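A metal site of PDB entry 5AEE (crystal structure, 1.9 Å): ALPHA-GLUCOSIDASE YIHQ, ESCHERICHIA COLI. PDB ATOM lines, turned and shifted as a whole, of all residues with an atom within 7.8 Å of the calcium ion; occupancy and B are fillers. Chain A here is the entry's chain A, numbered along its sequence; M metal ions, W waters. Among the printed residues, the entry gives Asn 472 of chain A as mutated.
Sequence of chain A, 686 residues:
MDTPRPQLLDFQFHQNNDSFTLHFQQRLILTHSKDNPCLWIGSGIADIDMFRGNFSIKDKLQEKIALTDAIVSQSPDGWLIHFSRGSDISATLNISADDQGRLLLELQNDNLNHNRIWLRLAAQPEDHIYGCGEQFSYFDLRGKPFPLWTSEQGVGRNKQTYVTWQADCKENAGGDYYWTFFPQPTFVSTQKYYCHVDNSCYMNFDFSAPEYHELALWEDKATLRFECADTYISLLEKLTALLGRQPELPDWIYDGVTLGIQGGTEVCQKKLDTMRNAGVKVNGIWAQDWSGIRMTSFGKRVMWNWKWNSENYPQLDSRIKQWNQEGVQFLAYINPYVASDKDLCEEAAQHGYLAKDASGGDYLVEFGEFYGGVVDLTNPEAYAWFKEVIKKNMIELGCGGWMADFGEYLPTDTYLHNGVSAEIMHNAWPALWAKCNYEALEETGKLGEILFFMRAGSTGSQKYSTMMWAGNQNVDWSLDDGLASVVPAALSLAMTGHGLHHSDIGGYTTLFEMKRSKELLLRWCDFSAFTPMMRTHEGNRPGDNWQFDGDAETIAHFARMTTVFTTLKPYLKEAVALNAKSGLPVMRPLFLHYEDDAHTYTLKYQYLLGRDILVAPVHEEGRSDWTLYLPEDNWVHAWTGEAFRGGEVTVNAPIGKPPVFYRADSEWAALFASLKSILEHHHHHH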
ATOM      1  N   PHE A 136     -16.210  -5.742  17.763  1.00  0.00           N
ATOM      2  CA  PHE A 136     -15.574  -6.949  17.202  1.00  0.00           C
ATOM      3  C   PHE A 136     -16.516  -7.788  16.391  1.00  0.00           C
ATOM      4  O   PHE A 136     -16.086  -8.521  15.550  1.00  0.00           O
ATOM      5  CB  PHE A 136     -14.980  -7.774  18.316  1.00  0.00           C
ATOM      6  CG  PHE A 136     -13.738  -7.156  18.902  1.00  0.00           C
ATOM      7  CD1 PHE A 136     -13.844  -6.193  19.870  1.00  0.00           C
ATOM      8  CD2 PHE A 136     -12.526  -7.522  18.455  1.00  0.00           C
ATOM      9  CE1 PHE A 136     -12.707  -5.550  20.371  1.00  0.00           C
ATOM     10  CE2 PHE A 136     -11.392  -6.948  18.969  1.00  0.00           C
ATOM     11  CZ  PHE A 136     -11.491  -5.968  19.921  1.00  0.00           C
ATOM     12  N   GLU A 152     -14.040  -7.265  30.104  1.00  0.00           N
ATOM     13  CA  GLU A 152     -13.425  -8.292  29.238  1.00  0.00           C
ATOM     14  C   GLU A 152     -14.232  -8.499  27.988  1.00  0.00           C
ATOM     15  O   GLU A 152     -15.451  -8.391  27.936  1.00  0.00           O
ATOM     16  CB  GLU A 152     -13.223  -9.648  29.902  1.00  0.00           C
ATOM     17  CG  GLU A 152     -12.471  -9.634  31.218  1.00  0.00           C
ATOM     18  CD  GLU A 152     -11.157  -8.840  31.156  1.00  0.00           C
ATOM     19  OE1 GLU A 152     -10.276  -9.208  30.351  1.00  0.00           O
ATOM     20  OE2 GLU A 152     -11.062  -7.806  31.903  1.00  0.00           O
ATOM     21  N   GLN A 153     -13.507  -8.740  26.937  1.00  0.00           N
ATOM     22  CA  GLN A 153     -14.052  -8.781  25.582  1.00  0.00           C
ATOM     23  C   GLN A 153     -14.869 -10.071  25.243  1.00  0.00           C
ATOM     24  O   GLN A 153     -15.584 -10.094  24.255  1.00  0.00           O
ATOM     25  CB  GLN A 153     -12.887  -8.601  24.665  1.00  0.00           C
ATOM     26  CG  GLN A 153     -13.216  -8.351  23.246  1.00  0.00           C
ATOM     27  CD  GLN A 153     -12.748  -9.450  22.374  1.00  0.00           C
ATOM     28  OE1 GLN A 153     -12.407 -10.578  22.805  1.00  0.00           O
ATOM     29  NE2 GLN A 153     -12.793  -9.168  21.104  1.00  0.00           N
ATOM     30  N   GLY A 154     -14.758 -11.117  26.060  1.00  0.00           N
ATOM     31  CA  GLY A 154     -15.396 -12.379  25.726  1.00  0.00           C
ATOM     32  C   GLY A 154     -14.429 -13.388  25.138  1.00  0.00           C
ATOM     33  O   GLY A 154     -13.563 -13.047  24.348  1.00  0.00           O
ATOM     34  N   VAL A 155     -14.660 -14.643  25.473  1.00  0.00           N
ATOM     35  CA  VAL A 155     -13.991 -15.775  24.868  1.00  0.00           C
ATOM     36  C   VAL A 155     -14.993 -16.533  24.006  1.00  0.00           C
ATOM     37  O   VAL A 155     -15.775 -17.291  24.555  1.00  0.00           O
ATOM     38  CB  VAL A 155     -13.401 -16.727  25.929  1.00  0.00           C
ATOM     39  CG1 VAL A 155     -12.864 -17.971  25.277  1.00  0.00           C
ATOM     40  CG2 VAL A 155     -12.337 -15.996  26.753  1.00  0.00           C
ATOM     41  N   GLY A 156     -14.952 -16.331  22.684  1.00  0.00           N
ATOM     42  CA  GLY A 156     -15.991 -16.910  21.796  1.00  0.00           C
ATOM     43  C   GLY A 156     -16.970 -15.863  21.310  1.00  0.00           C
ATOM     44  O   GLY A 156     -17.124 -15.618  20.105  1.00  0.00           O
ATOM     45  N   ARG A 157     -17.591 -15.179  22.255  1.00  0.00           N
ATOM     46  CA  ARG A 157     -18.406 -13.942  22.001  1.00  0.00           C
ATOM     47  C   ARG A 157     -19.684 -14.236  21.239  1.00  0.00           C
ATOM     48  O   ARG A 157     -20.326 -13.297  20.794  1.00  0.00           O
ATOM     49  CB  ARG A 157     -17.634 -12.872  21.231  1.00  0.00           C
ATOM     50  CG  ARG A 157     -16.277 -12.630  21.948  1.00  0.00           C
ATOM     51  CD  ARG A 157     -15.453 -11.554  21.334  1.00  0.00           C
ATOM     52  NE  ARG A 157     -16.182 -10.265  21.515  1.00  0.00           N
ATOM     53  CZ  ARG A 157     -16.961  -9.690  20.629  1.00  0.00           C
ATOM     54  NH1 ARG A 157     -17.076 -10.202  19.416  1.00  0.00           N
ATOM     55  NH2 ARG A 157     -17.606  -8.546  20.927  1.00  0.00           N
ATOM     56  N   ALA A 173     -17.724 -16.212  30.991  1.00  0.00           N
ATOM     57  CA  ALA A 173     -16.633 -15.534  30.305  1.00  0.00           C
ATOM     58  C   ALA A 173     -16.760 -15.546  28.755  1.00  0.00           C
ATOM     59  O   ALA A 173     -15.909 -15.010  28.025  1.00  0.00           O
ATOM     60  CB  ALA A 173     -15.304 -16.096  30.745  1.00  0.00           C
ATOM     61  N   GLY A 174     -17.839 -16.093  28.237  1.00  0.00           N
ATOM     62  CA  GLY A 174     -17.978 -16.198  26.788  1.00  0.00           C
ATOM     63  C   GLY A 174     -18.309 -14.895  26.101  1.00  0.00           C
ATOM     64  O   GLY A 174     -17.874 -14.619  24.969  1.00  0.00           O
ATOM     65  N   PHE A 181     -13.603  -4.020  25.671  1.00  0.00           N
ATOM     66  CA  PHE A 181     -12.833  -3.262  26.608  1.00  0.00           C
ATOM     67  C   PHE A 181     -12.721  -1.774  26.190  1.00  0.00           C
ATOM     68  O   PHE A 181     -12.165  -0.950  26.930  1.00  0.00           O
ATOM     69  CB  PHE A 181     -11.405  -3.863  26.769  1.00  0.00           C
ATOM     70  CG  PHE A 181     -10.881  -4.438  25.544  1.00  0.00           C
ATOM     71  CD1 PHE A 181     -10.666  -3.649  24.421  1.00  0.00           C
ATOM     72  CD2 PHE A 181     -10.601  -5.777  25.479  1.00  0.00           C
ATOM     73  CE1 PHE A 181     -10.198  -4.224  23.258  1.00  0.00           C
ATOM     74  CE2 PHE A 181     -10.128  -6.335  24.341  1.00  0.00           C
ATOM     75  CZ  PHE A 181      -9.917  -5.567  23.213  1.00  0.00           C
ATOM     76  N   ALA A 470      -5.773  -5.126  19.521  1.00  0.00           N
ATOM     77  CA  ALA A 470      -7.115  -5.732  19.527  1.00  0.00           C
ATOM     78  C   ALA A 470      -7.419  -6.698  20.699  1.00  0.00           C
ATOM     79  O   ALA A 470      -8.495  -7.360  20.677  1.00  0.00           O
ATOM     80  CB  ALA A 470      -7.379  -6.441  18.205  1.00  0.00           C
ATOM     81  N   GLY A 471      -6.598  -6.729  21.723  1.00  0.00           N
ATOM     82  CA  GLY A 471      -6.875  -7.524  22.886  1.00  0.00           C
ATOM     83  C   GLY A 471      -6.790  -9.001  22.521  1.00  0.00           C
ATOM     84  O   GLY A 471      -6.045  -9.386  21.630  1.00  0.00           O
ATOM     85  N   ASN A 472      -7.581  -9.820  23.168  1.00  0.00           N
ATOM     86  CA  ASN A 472      -7.422 -11.289  23.103  1.00  0.00           C
ATOM     87  C   ASN A 472      -8.391 -11.923  22.169  1.00  0.00           C
ATOM     88  O   ASN A 472      -9.585 -12.029  22.517  1.00  0.00           O
ATOM     89  CB  ASN A 472      -7.624 -11.838  24.513  1.00  0.00           C
ATOM     90  CG  ASN A 472      -6.551 -11.440  25.479  1.00  0.00           C
ATOM     91  OD1 ASN A 472      -5.516 -10.889  25.101  1.00  0.00           O
ATOM     92  ND2 ASN A 472      -6.794 -11.726  26.740  1.00  0.00           N
ATOM     93  N   GLN A 473      -7.904 -12.254  20.996  1.00  0.00           N
ATOM     94  CA  GLN A 473      -8.549 -13.179  20.097  1.00  0.00           C
ATOM     95  C   GLN A 473      -8.245 -14.598  20.538  1.00  0.00           C
ATOM     96  O   GLN A 473      -7.176 -14.959  20.950  1.00  0.00           O
ATOM     97  CB  GLN A 473      -8.078 -13.046  18.640  1.00  0.00           C
ATOM     98  CG  GLN A 473      -8.674 -11.838  17.953  1.00  0.00           C
ATOM     99  CD  GLN A 473      -8.147 -10.551  18.480  1.00  0.00           C
ATOM    100  OE1 GLN A 473      -6.935 -10.254  18.366  1.00  0.00           O
ATOM    101  NE2 GLN A 473      -9.031  -9.778  19.079  1.00  0.00           N
ATOM    102  N   ASN A 474      -9.239 -15.446  20.324  1.00  0.00           N
ATOM    103  CA  ASN A 474      -9.012 -16.876  20.350  1.00  0.00           C
ATOM    104  C   ASN A 474      -8.046 -17.244  19.307  1.00  0.00           C
ATOM    105  O   ASN A 474      -8.016 -16.628  18.235  1.00  0.00           O
ATOM    106  CB  ASN A 474     -10.349 -17.632  20.071  1.00  0.00           C
ATOM    107  CG  ASN A 474     -11.335 -17.518  21.205  1.00  0.00           C
ATOM    108  OD1 ASN A 474     -10.972 -17.172  22.300  1.00  0.00           O
ATOM    109  ND2 ASN A 474     -12.599 -17.981  20.989  1.00  0.00           N
ATOM    110  N   ASP A 480     -16.467 -14.080  15.308  1.00  0.00           N
ATOM    111  CA  ASP A 480     -16.663 -13.161  16.431  1.00  0.00           C
ATOM    112  C   ASP A 480     -15.429 -13.044  17.334  1.00  0.00           C
ATOM    113  O   ASP A 480     -15.379 -12.110  18.086  1.00  0.00           O
ATOM    114  CB  ASP A 480     -17.815 -13.569  17.290  1.00  0.00           C
ATOM    115  CG  ASP A 480     -19.156 -13.478  16.545  1.00  0.00           C
ATOM    116  OD1 ASP A 480     -19.736 -12.388  16.499  1.00  0.00           O
ATOM    117  OD2 ASP A 480     -19.573 -14.518  16.007  1.00  0.00           O
ATOM    118  N   ASP A 481     -14.509 -14.030  17.310  1.00  0.00           N
ATOM    119  CA  ASP A 481     -13.342 -13.927  18.189  1.00  0.00           C
ATOM    120  C   ASP A 481     -12.002 -14.399  17.630  1.00  0.00           C
ATOM    121  O   ASP A 481     -11.068 -14.519  18.373  1.00  0.00           O
ATOM    122  CB  ASP A 481     -13.654 -14.593  19.520  1.00  0.00           C
ATOM    123  CG  ASP A 481     -12.908 -13.953  20.726  1.00  0.00           C
ATOM    124  OD1 ASP A 481     -12.261 -12.866  20.623  1.00  0.00           O
ATOM    125  OD2 ASP A 481     -12.940 -14.572  21.849  1.00  0.00           O
ATOM    126  N   GLY A 482     -11.918 -14.553  16.321  1.00  0.00           N
ATOM    127  CA  GLY A 482     -10.722 -15.009  15.665  1.00  0.00           C
ATOM    128  C   GLY A 482     -10.160 -13.845  14.881  1.00  0.00           C
ATOM    129  O   GLY A 482     -10.530 -12.666  15.092  1.00  0.00           O
ATOM    130  N   SER A 485     -12.204 -10.861  13.393  1.00  0.00           N
ATOM    131  CA  SER A 485     -12.833  -9.863  14.273  1.00  0.00           C
ATOM    132  C   SER A 485     -11.969  -8.676  14.440  1.00  0.00           C
ATOM    133  O   SER A 485     -12.427  -7.591  14.835  1.00  0.00           O
ATOM    134  CB  SER A 485     -13.150 -10.480  15.657  1.00  0.00           C
ATOM    135  OG  SER A 485     -12.009 -10.931  16.334  1.00  0.00           O
ATOM    136  N   TYR A 508      -4.384 -14.953  20.877  1.00  0.00           N
ATOM    137  CA  TYR A 508      -3.909 -15.117  22.244  1.00  0.00           C
ATOM    138  C   TYR A 508      -4.502 -16.279  23.029  1.00  0.00           C
ATOM    139  O   TYR A 508      -3.758 -17.108  23.532  1.00  0.00           O
ATOM    140  CB  TYR A 508      -4.112 -13.796  23.046  1.00  0.00           C
ATOM    141  CG  TYR A 508      -3.775 -13.927  24.505  1.00  0.00           C
ATOM    142  CD1 TYR A 508      -2.485 -13.801  24.935  1.00  0.00           C
ATOM    143  CD2 TYR A 508      -4.769 -14.171  25.445  1.00  0.00           C
ATOM    144  CE1 TYR A 508      -2.185 -13.893  26.290  1.00  0.00           C
ATOM    145  CE2 TYR A 508      -4.482 -14.292  26.814  1.00  0.00           C
ATOM    146  CZ  TYR A 508      -3.173 -14.119  27.245  1.00  0.00           C
ATOM    147  OH  TYR A 508      -2.825 -14.274  28.605  1.00  0.00           O
ATOM    148  N   THR A 509      -5.844 -16.345  23.059  1.00  0.00           N
ATOM    149  CA  THR A 509      -6.565 -17.137  23.970  1.00  0.00           C
ATOM    150  C   THR A 509      -6.562 -18.613  23.595  1.00  0.00           C
ATOM    151  O   THR A 509      -7.038 -19.014  22.550  1.00  0.00           O
ATOM    152  CB  THR A 509      -8.020 -16.648  24.091  1.00  0.00           C
ATOM    153  OG1 THR A 509      -8.015 -15.217  24.361  1.00  0.00           O
ATOM    154  CG2 THR A 509      -8.762 -17.488  25.248  1.00  0.00           C
HETATM  155 CA    CA M   1     -11.711 -12.709  22.988  1.00  0.00          CA
HETATM  156  O   HOH W   1     -10.486 -14.707  23.282  1.00  0.00           O
HETATM  157  O   HOH W   2     -11.088 -12.088  25.172  1.00  0.00           O
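Four residues have an atom within 4 Å of the calcium ion: Gln 153, Gly 154, Asn 472 and Asp 481.
Along chain A the residues within 4 Å of the calcium ion span positions 153 to 481.
The calcium ion is bound by the side-chain amide oxygen (OE1) of Gln 153 (2.2 Å), the backbone carbonyl oxygen (O) of Asn 472 (2.3 Å), the backbone carbonyl oxygen (O) of Gly 154 (2.3 Å), water W2 (2.4 Å), water W1 (2.4 Å), the side-chain carboxylate (OD1) of Asp 481 (2.4 Å) and the side-chain carboxylate (OD2) of Asp 481 (2.5 Å).
The calcium ion has seven donor atoms within binding distance.
The backbone carbonyl oxygen (O) of Gln 153 sits at hydrogen-bond distance from the guanidinium group (NE) of Arg 157, 2.8 Å away.
The backbone NH (N) of Asn 474 lies within hydrogen-bond range of the backbone carbonyl oxygen (O) of Asp 481 (2.8 Å).
N of Gly 156 sits close to OD2 of Asp 481.
Water W1 bridges OD1 of Asn 474 (2.7 Å) and OG1 of Thr 509 (2.7 Å).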
